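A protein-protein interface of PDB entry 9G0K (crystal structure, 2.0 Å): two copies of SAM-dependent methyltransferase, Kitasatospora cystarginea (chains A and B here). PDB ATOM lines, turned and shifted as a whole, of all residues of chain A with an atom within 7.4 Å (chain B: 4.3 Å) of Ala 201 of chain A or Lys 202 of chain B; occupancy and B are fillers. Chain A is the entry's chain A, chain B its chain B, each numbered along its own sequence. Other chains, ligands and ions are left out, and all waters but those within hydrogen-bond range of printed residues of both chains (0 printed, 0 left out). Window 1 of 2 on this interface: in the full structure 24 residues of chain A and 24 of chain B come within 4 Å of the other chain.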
ATOM      1  N   SER A  14     -10.754  -0.255   7.719  1.00  0.00           N
ATOM      2  CA  SER A  14     -11.778  -1.007   8.496  1.00  0.00           C
ATOM      3  C   SER A  14     -13.072  -0.197   8.616  1.00  0.00           C
ATOM      4  O   SER A  14     -13.632  -0.093   9.771  1.00  0.00           O
ATOM      5  CB  SER A  14     -11.271  -1.325   9.850  1.00  0.00           C
ATOM      6  OG  SER A  14     -10.222  -2.247   9.750  1.00  0.00           O
ATOM      7  N   LEU A  17     -16.181  -2.058  10.096  1.00  0.00           N
ATOM      8  CA  LEU A  17     -15.941  -2.366  11.519  1.00  0.00           C
ATOM      9  C   LEU A  17     -16.205  -1.107  12.349  1.00  0.00           C
ATOM     10  O   LEU A  17     -16.896  -1.182  13.391  1.00  0.00           O
ATOM     11  CB  LEU A  17     -14.473  -2.770  11.701  1.00  0.00           C
ATOM     12  CG  LEU A  17     -14.040  -2.862  13.166  1.00  0.00           C
ATOM     13  CD1 LEU A  17     -14.894  -3.950  13.879  1.00  0.00           C
ATOM     14  CD2 LEU A  17     -12.530  -3.120  13.272  1.00  0.00           C
ATOM     15  N   LEU A  18     -15.635   0.026  11.932  1.00  0.00           N
ATOM     16  CA  LEU A  18     -15.582   1.218  12.815  1.00  0.00           C
ATOM     17  C   LEU A  18     -16.942   1.919  12.750  1.00  0.00           C
ATOM     18  O   LEU A  18     -17.489   2.233  13.853  1.00  0.00           O
ATOM     19  CB  LEU A  18     -14.409   2.090  12.399  1.00  0.00           C
ATOM     20  CG  LEU A  18     -13.065   1.389  12.609  1.00  0.00           C
ATOM     21  CD1 LEU A  18     -11.937   2.110  11.934  1.00  0.00           C
ATOM     22  CD2 LEU A  18     -12.748   1.268  14.066  1.00  0.00           C
ATOM     23  N   TYR A  19     -17.509   2.103  11.548  1.00  0.00           N
ATOM     24  CA  TYR A  19     -18.840   2.743  11.399  1.00  0.00           C
ATOM     25  C   TYR A  19     -19.901   1.845  12.015  1.00  0.00           C
ATOM     26  O   TYR A  19     -20.749   2.401  12.835  1.00  0.00           O
ATOM     27  CB  TYR A  19     -19.147   3.112   9.959  1.00  0.00           C
ATOM     28  CG  TYR A  19     -18.618   4.498   9.644  1.00  0.00           C
ATOM     29  CD1 TYR A  19     -19.465   5.572   9.497  1.00  0.00           C
ATOM     30  CD2 TYR A  19     -17.292   4.694   9.371  1.00  0.00           C
ATOM     31  CE1 TYR A  19     -18.987   6.822   9.159  1.00  0.00           C
ATOM     32  CE2 TYR A  19     -16.785   5.943   9.095  1.00  0.00           C
ATOM     33  CZ  TYR A  19     -17.642   7.005   8.947  1.00  0.00           C
ATOM     34  OH  TYR A  19     -17.165   8.239   8.581  1.00  0.00           O
ATOM     35  N   SER A  21     -19.532  -0.283  14.331  1.00  0.00           N
ATOM     36  CA  SER A  21     -19.432  -0.391  15.798  1.00  0.00           C
ATOM     37  C   SER A  21     -20.145   0.807  16.388  1.00  0.00           C
ATOM     38  O   SER A  21     -20.750   0.652  17.427  1.00  0.00           O
ATOM     39  CB  SER A  21     -18.001  -0.555  16.250  1.00  0.00           C
ATOM     40  OG  SER A  21     -17.526  -1.880  15.920  1.00  0.00           O
ATOM     41  N   ALA A  22     -20.185   1.935  15.678  1.00  0.00           N
ATOM     42  CA  ALA A  22     -20.924   3.118  16.172  1.00  0.00           C
ATOM     43  C   ALA A  22     -22.432   2.865  16.084  1.00  0.00           C
ATOM     44  O   ALA A  22     -23.157   3.255  16.993  1.00  0.00           O
ATOM     45  CB  ALA A  22     -20.516   4.342  15.385  1.00  0.00           C
ATOM     46  N   ASN A 134     -17.977   8.538  19.059  1.00  0.00           N
ATOM     47  CA  ASN A 134     -17.061   9.217  18.127  1.00  0.00           C
ATOM     48  C   ASN A 134     -16.284   8.197  17.330  1.00  0.00           C
ATOM     49  O   ASN A 134     -15.588   7.387  17.951  1.00  0.00           O
ATOM     50  CB  ASN A 134     -16.006  10.067  18.844  1.00  0.00           C
ATOM     51  CG  ASN A 134     -15.384  11.080  17.927  1.00  0.00           C
ATOM     52  OD1 ASN A 134     -15.710  11.085  16.720  1.00  0.00           O
ATOM     53  ND2 ASN A 134     -14.467  11.885  18.483  1.00  0.00           N
ATOM     54  N   GLU A 136     -13.168   8.251  14.950  1.00  0.00           N
ATOM     55  CA  GLU A 136     -12.225   9.384  15.073  1.00  0.00           C
ATOM     56  C   GLU A 136     -10.862   9.000  14.537  1.00  0.00           C
ATOM     57  O   GLU A 136     -10.427   7.839  14.768  1.00  0.00           O
ATOM     58  CB  GLU A 136     -12.127   9.902  16.516  1.00  0.00           C
ATOM     59  CG  GLU A 136     -11.399  11.251  16.604  1.00  0.00           C
ATOM     60  CD  GLU A 136     -11.939  12.358  15.708  1.00  0.00           C
ATOM     61  OE1 GLU A 136     -12.501  13.368  16.237  1.00  0.00           O
ATOM     62  OE2 GLU A 136     -11.741  12.251  14.475  1.00  0.00           O
ATOM     63  N   VAL A 182      -6.045   8.146  21.608  1.00  0.00           N
ATOM     64  CA  VAL A 182      -7.437   7.762  21.921  1.00  0.00           C
ATOM     65  C   VAL A 182      -7.639   7.713  23.448  1.00  0.00           C
ATOM     66  O   VAL A 182      -8.738   8.074  23.878  1.00  0.00           O
ATOM     67  CB  VAL A 182      -7.787   6.445  21.218  1.00  0.00           C
ATOM     68  CG1 VAL A 182      -7.040   5.228  21.790  1.00  0.00           C
ATOM     69  CG2 VAL A 182      -9.290   6.285  21.224  1.00  0.00           C
ATOM     70  N   ASP A 198     -15.242   4.013  26.803  1.00  0.00           N
ATOM     71  CA  ASP A 198     -14.568   2.778  26.326  1.00  0.00           C
ATOM     72  C   ASP A 198     -14.160   2.928  24.857  1.00  0.00           C
ATOM     73  O   ASP A 198     -14.846   3.644  24.108  1.00  0.00           O
ATOM     74  CB  ASP A 198     -15.471   1.548  26.518  1.00  0.00           C
ATOM     75  CG  ASP A 198     -14.721   0.240  26.289  1.00  0.00           C
ATOM     76  OD1 ASP A 198     -13.563   0.215  26.574  1.00  0.00           O
ATOM     77  OD2 ASP A 198     -15.313  -0.730  25.783  1.00  0.00           O
ATOM     78  N   CYS A 199     -13.045   2.307  24.463  1.00  0.00           N
ATOM     79  CA  CYS A 199     -12.651   2.239  23.036  1.00  0.00           C
ATOM     80  C   CYS A 199     -13.178   0.933  22.490  1.00  0.00           C
ATOM     81  O   CYS A 199     -12.602  -0.081  22.927  1.00  0.00           O
ATOM     82  CB  CYS A 199     -11.154   2.211  22.837  1.00  0.00           C
ATOM     83  SG  CYS A 199     -10.640   2.086  21.121  1.00  0.00           S
ATOM     84  N   LEU A 200     -14.208   0.960  21.631  1.00  0.00           N
ATOM     85  CA  LEU A 200     -14.929  -0.264  21.192  1.00  0.00           C
ATOM     86  C   LEU A 200     -14.136  -0.987  20.104  1.00  0.00           C
ATOM     87  O   LEU A 200     -13.872  -2.238  20.222  1.00  0.00           O
ATOM     88  CB  LEU A 200     -16.292   0.154  20.674  1.00  0.00           C
ATOM     89  CG  LEU A 200     -17.138   0.896  21.705  1.00  0.00           C
ATOM     90  CD1 LEU A 200     -18.385   1.439  21.033  1.00  0.00           C
ATOM     91  CD2 LEU A 200     -17.511  -0.017  22.857  1.00  0.00           C
ATOM     92  N   ALA A 201     -13.696  -0.242  19.102  1.00  0.00           N
ATOM     93  CA  ALA A 201     -12.981  -0.865  17.968  1.00  0.00           C
ATOM     94  C   ALA A 201     -11.869   0.062  17.524  1.00  0.00           C
ATOM     95  O   ALA A 201     -12.039   1.317  17.802  1.00  0.00           O
ATOM     96  CB  ALA A 201     -13.952  -1.155  16.869  1.00  0.00           C
ATOM     97  N   LYS A 202     -10.797  -0.473  16.932  1.00  0.00           N
ATOM     98  CA  LYS A 202      -9.627   0.335  16.504  1.00  0.00           C
ATOM     99  C   LYS A 202      -8.900  -0.305  15.358  1.00  0.00           C
ATOM    100  O   LYS A 202      -8.733  -1.500  15.418  1.00  0.00           O
ATOM    101  CB  LYS A 202      -8.600   0.460  17.615  1.00  0.00           C
ATOM    102  CG  LYS A 202      -7.523   1.555  17.427  1.00  0.00           C
ATOM    103  CD  LYS A 202      -6.877   1.942  18.763  1.00  0.00           C
ATOM    104  CE  LYS A 202      -5.970   3.154  18.755  1.00  0.00           C
ATOM    105  NZ  LYS A 202      -4.671   2.840  18.104  1.00  0.00           N
ATOM    106  N   ASP A 203      -8.460   0.476  14.402  1.00  0.00           N
ATOM    107  CA  ASP A 203      -7.509   0.061  13.336  1.00  0.00           C
ATOM    108  C   ASP A 203      -6.418   1.139  13.243  1.00  0.00           C
ATOM    109  O   ASP A 203      -6.531   2.022  12.369  1.00  0.00           O
ATOM    110  CB  ASP A 203      -8.254  -0.192  12.013  1.00  0.00           C
ATOM    111  CG  ASP A 203      -7.337  -0.735  10.942  1.00  0.00           C
ATOM    112  OD1 ASP A 203      -6.167  -0.626  11.201  1.00  0.00           O
ATOM    113  OD2 ASP A 203      -7.794  -1.290   9.868  1.00  0.00           O
ATOM    114  N   TRP A 204      -5.452   1.069  14.163  1.00  0.00           N
ATOM    115  CA  TRP A 204      -4.289   1.988  14.255  1.00  0.00           C
ATOM    116  C   TRP A 204      -4.744   3.453  14.379  1.00  0.00           C
ATOM    117  O   TRP A 204      -5.165   3.837  15.475  1.00  0.00           O
ATOM    118  CB  TRP A 204      -3.307   1.746  13.099  1.00  0.00           C
ATOM    119  CG  TRP A 204      -2.722   0.365  13.071  1.00  0.00           C
ATOM    120  CD1 TRP A 204      -3.375  -0.798  12.779  1.00  0.00           C
ATOM    121  CD2 TRP A 204      -1.359  -0.008  13.342  1.00  0.00           C
ATOM    122  NE1 TRP A 204      -2.521  -1.865  12.846  1.00  0.00           N
ATOM    123  CE2 TRP A 204      -1.277  -1.412  13.193  1.00  0.00           C
ATOM    124  CE3 TRP A 204      -0.205   0.700  13.696  1.00  0.00           C
ATOM    125  CZ2 TRP A 204      -0.088  -2.112  13.382  1.00  0.00           C
ATOM    126  CZ3 TRP A 204       0.968   0.006  13.887  1.00  0.00           C
ATOM    127  CH2 TRP A 204       1.023  -1.381  13.730  1.00  0.00           C
ATOM    128  N   PHE A 206      -7.417   4.915  13.279  1.00  0.00           N
ATOM    129  CA  PHE A 206      -8.879   5.144  13.414  1.00  0.00           C
ATOM    130  C   PHE A 206      -9.463   4.289  14.543  1.00  0.00           C
ATOM    131  O   PHE A 206      -9.050   3.125  14.701  1.00  0.00           O
ATOM    132  CB  PHE A 206      -9.555   5.005  12.051  1.00  0.00           C
ATOM    133  CG  PHE A 206      -8.987   5.945  11.020  1.00  0.00           C
ATOM    134  CD1 PHE A 206      -9.515   7.214  10.847  1.00  0.00           C
ATOM    135  CD2 PHE A 206      -7.892   5.580  10.255  1.00  0.00           C
ATOM    136  CE1 PHE A 206      -8.983   8.082   9.908  1.00  0.00           C
ATOM    137  CE2 PHE A 206      -7.359   6.449   9.318  1.00  0.00           C
ATOM    138  CZ  PHE A 206      -7.904   7.699   9.147  1.00  0.00           C
ATOM    139  N   ALA A 207     -10.404   4.863  15.297  1.00  0.00           N
ATOM    140  CA  ALA A 207     -11.022   4.175  16.445  1.00  0.00           C
ATOM    141  C   ALA A 207     -12.457   4.670  16.631  1.00  0.00           C
ATOM    142  O   ALA A 207     -12.738   5.860  16.348  1.00  0.00           O
ATOM    143  CB  ALA A 207     -10.248   4.442  17.691  1.00  0.00           C
ATOM    144  N   THR A 208     -13.308   3.801  17.165  1.00  0.00           N
ATOM    145  CA  THR A 208     -14.655   4.123  17.672  1.00  0.00           C
ATOM    146  C   THR A 208     -14.646   4.089  19.199  1.00  0.00           C
ATOM    147  O   THR A 208     -14.499   3.007  19.841  1.00  0.00           O
ATOM    148  CB  THR A 208     -15.617   3.133  17.034  1.00  0.00           C
ATOM    149  OG1 THR A 208     -15.414   3.310  15.652  1.00  0.00           O
ATOM    150  CG2 THR A 208     -17.044   3.461  17.287  1.00  0.00           C
ATOM    151  N   TYR A 209     -14.789   5.233  19.832  1.00  0.00           N
ATOM    152  CA  TYR A 209     -14.974   5.267  21.310  1.00  0.00           C
ATOM    153  C   TYR A 209     -16.344   5.825  21.666  1.00  0.00           C
ATOM    154  O   TYR A 209     -17.043   6.464  20.795  1.00  0.00           O
ATOM    155  CB  TYR A 209     -13.816   5.981  21.988  1.00  0.00           C
ATOM    156  CG  TYR A 209     -13.668   7.438  21.656  1.00  0.00           C
ATOM    157  CD1 TYR A 209     -14.238   8.395  22.451  1.00  0.00           C
ATOM    158  CD2 TYR A 209     -12.839   7.860  20.647  1.00  0.00           C
ATOM    159  CE1 TYR A 209     -14.047   9.761  22.206  1.00  0.00           C
ATOM    160  CE2 TYR A 209     -12.662   9.222  20.378  1.00  0.00           C
ATOM    161  CZ  TYR A 209     -13.260  10.173  21.162  1.00  0.00           C
ATOM    162  OH  TYR A 209     -13.093  11.504  20.884  1.00  0.00           O
ATOM    163  N   LEU B  18      -6.489  -8.539  13.300  1.00  0.00           N
ATOM    164  CA  LEU B  18      -5.894  -8.641  14.654  1.00  0.00           C
ATOM    165  C   LEU B  18      -4.576  -9.387  14.568  1.00  0.00           C
ATOM    166  O   LEU B  18      -3.537  -8.839  15.054  1.00  0.00           O
ATOM    167  CB  LEU B  18      -6.881  -9.310  15.600  1.00  0.00           C
ATOM    168  CG  LEU B  18      -8.072  -8.427  15.933  1.00  0.00           C
ATOM    169  CD1 LEU B  18      -8.989  -9.175  16.824  1.00  0.00           C
ATOM    170  CD2 LEU B  18      -7.623  -7.085  16.616  1.00  0.00           C
ATOM    171  N   TYR B 149     -20.158  -6.599  24.406  1.00  0.00           N
ATOM    172  CA  TYR B 149     -18.986  -7.292  23.812  1.00  0.00           C
ATOM    173  C   TYR B 149     -19.437  -8.724  23.414  1.00  0.00           C
ATOM    174  O   TYR B 149     -19.070  -9.220  22.387  1.00  0.00           O
ATOM    175  CB  TYR B 149     -17.843  -7.376  24.814  1.00  0.00           C
ATOM    176  CG  TYR B 149     -16.932  -6.180  24.934  1.00  0.00           C
ATOM    177  CD1 TYR B 149     -15.583  -6.380  25.140  1.00  0.00           C
ATOM    178  CD2 TYR B 149     -17.409  -4.872  24.977  1.00  0.00           C
ATOM    179  CE1 TYR B 149     -14.712  -5.323  25.249  1.00  0.00           C
ATOM    180  CE2 TYR B 149     -16.550  -3.796  25.156  1.00  0.00           C
ATOM    181  CZ  TYR B 149     -15.191  -4.024  25.294  1.00  0.00           C
ATOM    182  OH  TYR B 149     -14.302  -2.995  25.480  1.00  0.00           O
ATOM    183  N   VAL B 182      -8.555  -4.146  28.454  1.00  0.00           N
ATOM    184  CA  VAL B 182      -7.311  -3.924  27.696  1.00  0.00           C
ATOM    185  C   VAL B 182      -6.451  -2.800  28.333  1.00  0.00           C
ATOM    186  O   VAL B 182      -5.217  -2.945  28.278  1.00  0.00           O
ATOM    187  CB  VAL B 182      -7.674  -3.699  26.220  1.00  0.00           C
ATOM    188  CG1 VAL B 182      -8.300  -2.325  25.955  1.00  0.00           C
ATOM    189  CG2 VAL B 182      -6.457  -3.934  25.362  1.00  0.00           C
ATOM    190  N   CYS B 199      -2.451   0.110  22.256  1.00  0.00           N
ATOM    191  CA  CYS B 199      -3.438  -0.837  21.677  1.00  0.00           C
ATOM    192  C   CYS B 199      -3.518  -0.519  20.195  1.00  0.00           C
ATOM    193  O   CYS B 199      -3.927   0.573  19.852  1.00  0.00           O
ATOM    194  CB  CYS B 199      -4.826  -0.678  22.275  1.00  0.00           C
ATOM    195  SG  CYS B 199      -6.071  -1.754  21.519  1.00  0.00           S
ATOM    196  N   ALA B 201      -4.988  -2.394  17.439  1.00  0.00           N
ATOM    197  CA  ALA B 201      -6.275  -2.715  16.824  1.00  0.00           C
ATOM    198  C   ALA B 201      -7.128  -3.413  17.883  1.00  0.00           C
ATOM    199  O   ALA B 201      -6.567  -3.878  18.915  1.00  0.00           O
ATOM    200  CB  ALA B 201      -6.048  -3.554  15.591  1.00  0.00           C
ATOM    201  N   LYS B 202      -8.435  -3.424  17.639  1.00  0.00           N
ATOM    202  CA  LYS B 202      -9.445  -3.895  18.588  1.00  0.00           C
ATOM    203  C   LYS B 202     -10.771  -4.090  17.843  1.00  0.00           C
ATOM    204  O   LYS B 202     -11.045  -3.441  16.846  1.00  0.00           O
ATOM    205  CB  LYS B 202      -9.604  -2.893  19.735  1.00  0.00           C
ATOM    206  CG  LYS B 202     -10.506  -3.325  20.880  1.00  0.00           C
ATOM    207  CD  LYS B 202     -10.359  -2.381  22.123  1.00  0.00           C
ATOM    208  CE  LYS B 202     -11.171  -2.742  23.366  1.00  0.00           C
ATOM    209  NZ  LYS B 202     -12.629  -2.856  23.130  1.00  0.00           N
ATOM    210  N   ASP B 203     -11.527  -5.072  18.319  1.00  0.00           N
ATOM    211  CA  ASP B 203     -12.864  -5.437  17.814  1.00  0.00           C
ATOM    212  C   ASP B 203     -13.580  -5.942  19.052  1.00  0.00           C
ATOM    213  O   ASP B 203     -13.720  -7.206  19.218  1.00  0.00           O
ATOM    214  CB  ASP B 203     -12.803  -6.474  16.664  1.00  0.00           C
ATOM    215  CG  ASP B 203     -14.189  -6.773  16.136  1.00  0.00           C
ATOM    216  OD1 ASP B 203     -15.102  -6.142  16.638  1.00  0.00           O
ATOM    217  OD2 ASP B 203     -14.340  -7.622  15.219  1.00  0.00           O
ATOM    218  N   TRP B 204     -13.918  -5.025  19.925  1.00  0.00           N
ATOM    219  CA  TRP B 204     -14.694  -5.263  21.159  1.00  0.00           C
ATOM    220  C   TRP B 204     -13.881  -6.213  22.030  1.00  0.00           C
ATOM    221  O   TRP B 204     -12.957  -5.681  22.622  1.00  0.00           O
ATOM    222  CB  TRP B 204     -16.138  -5.690  20.854  1.00  0.00           C
ATOM    223  CG  TRP B 204     -16.959  -4.695  20.051  1.00  0.00           C
ATOM    224  CD1 TRP B 204     -16.907  -4.430  18.696  1.00  0.00           C
ATOM    225  CD2 TRP B 204     -18.068  -3.907  20.547  1.00  0.00           C
ATOM    226  NE1 TRP B 204     -17.835  -3.473  18.350  1.00  0.00           N
ATOM    227  CE2 TRP B 204     -18.566  -3.147  19.464  1.00  0.00           C
ATOM    228  CE3 TRP B 204     -18.688  -3.787  21.800  1.00  0.00           C
ATOM    229  CZ2 TRP B 204     -19.656  -2.313  19.610  1.00  0.00           C
ATOM    230  CZ3 TRP B 204     -19.738  -2.926  21.952  1.00  0.00           C
ATOM    231  CH2 TRP B 204     -20.223  -2.233  20.858  1.00  0.00           C
ATOM    232  N   PHE B 206     -11.790  -8.775  21.278  1.00  0.00           N
ATOM    233  CA  PHE B 206     -10.414  -9.089  20.828  1.00  0.00           C
ATOM    234  C   PHE B 206      -9.617  -7.812  20.478  1.00  0.00           C
ATOM    235  O   PHE B 206     -10.120  -6.904  19.839  1.00  0.00           O
ATOM    236  CB  PHE B 206     -10.562 -10.129  19.730  1.00  0.00           C
ATOM    237  CG  PHE B 206     -11.327 -11.353  20.196  1.00  0.00           C
ATOM    238  CD1 PHE B 206     -10.690 -12.316  20.959  1.00  0.00           C
ATOM    239  CD2 PHE B 206     -12.681 -11.481  19.947  1.00  0.00           C
ATOM    240  CE1 PHE B 206     -11.381 -13.402  21.428  1.00  0.00           C
ATOM    241  CE2 PHE B 206     -13.370 -12.549  20.466  1.00  0.00           C
ATOM    242  CZ  PHE B 206     -12.701 -13.544  21.140  1.00  0.00           C
ATOM    243  N   ALA B 207      -8.378  -7.730  20.950  1.00  0.00           N
ATOM    244  CA  ALA B 207      -7.494  -6.558  20.799  1.00  0.00           C
ATOM    245  C   ALA B 207      -6.067  -7.021  20.571  1.00  0.00           C
ATOM    246  O   ALA B 207      -5.702  -8.070  21.192  1.00  0.00           O
ATOM    247  CB  ALA B 207      -7.558  -5.773  22.053  1.00  0.00           C
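Printed residues of chain B that touch a printed residue of chain A: Tyr 149, Cys 199, Ala 201, Lys 202, Asp 203 and Trp 204. Hydrophobic or aromatic side chains of chain B within 4 Å of the printed part of chain A: Tyr 149, Ala 201 and Trp 204. Among the printed residues, no Asp or Glu carboxylate lies within 4 Å of a Lys or Arg side-chain nitrogen of the other chain.
Among the printed residues, merely in contact across the chains: Leu 17 of chain A with Lys 202 of chain B (3.9 Å), Leu 17 of chain A with Asp 203 of chain B (3.5 Å), Leu 200 of chain A with Asp 203 of chain B (3.9 Å), Ala 201 of chain A with Lys 202 of chain B (3.4 Å) and Lys 202 of chain A with Ala 201 of chain B (3.1 Å).
Of chain A, only Leu 17 (3.9 Å), Cys 199 (2.8 Å), Leu 200 (3.2 Å), Ala 201 (3.4 Å) and Lys 202 (3.0 Å) come within 4 Å of Lys 202 of chain B. Of the printed residues of chain A, Cys 199 of chain B touches Lys 202. Printed residues of chain A within 4 Å of Tyr 149 of chain B: Asp 198 (2.5 Å). Trp 204 of chain A touches none of the printed residues of chain B. The nearest printed residue of chain B that does not touch Ala 201 of chain A is Asp 203 of chain B (4.5 Å).
Cys 199 of chain A touches Lys 202 of chain B, and with the chains exchanged Lys 202 of chain A touches Cys 199 of chain B. Ala 201 of chain A touches Lys 202 of chain B, and with the chains exchanged Lys 202 of chain A touches Ala 201 of chain B. Lys 202 of chain B touches its own counterpart, Lys 202 of chain A. 9 positions are printed for both chains.
O of Ala 201 of chain A lies within hydrogen-bond range of N of Thr 208 of chain A. The side-chain sulfur of Cys 199 of chain A lies within hydrogen-bond range of the backbone carbonyl oxygen of Ala 201 of chain A (3.7 Å). N of Leu 200 of chain A is in hydrogen-bond range of O of Thr 208 of chain A, 2.7 Å away. The backbone carbonyl oxygen (O) of Leu 17 of chain A lies within hydrogen-bond range of the side-chain hydroxyl (OG) of Ser 21 of chain A, at 2.7 Å. The side-chain hydroxyl (OH) of Tyr 149 of chain B sits at hydrogen-bond distance from the side-chain amino group (NZ) of Lys 202 of chain B. NZ of Lys 202 of chain B is in hydrogen-bond range of O of Trp 204 of chain B (2.9 Å).
The side-chain amino group of Lys 202 of chain B is in hydrogen-bond range of the backbone carbonyl oxygen of Leu 200 of chain A. N of Lys 202 of chain B sits at hydrogen-bond distance from O of Lys 202 of chain A (3.0 Å). O of Cys 199 of chain B is in hydrogen-bond range of NZ of Lys 202 of chain A, at 3.0 Å. The backbone carbonyl oxygen (O) of Cys 199 of chain A lies within hydrogen-bond range of the side-chain amino group (NZ) of Lys 202 of chain B, at 2.8 Å. The side-chain carboxylate of Asp 198 of chain A sits at hydrogen-bond distance from the side-chain hydroxyl of Tyr 149 of chain B (2.5 Å). OG of Ser 21 of chain A lies within hydrogen-bond range of NE1 of Trp 204 of chain B (2.9 Å). The backbone carbonyl oxygen (O) of Leu 200 of chain A sits at hydrogen-bond distance from the backbone NH (N) of Trp 204 of chain B (2.8 Å).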
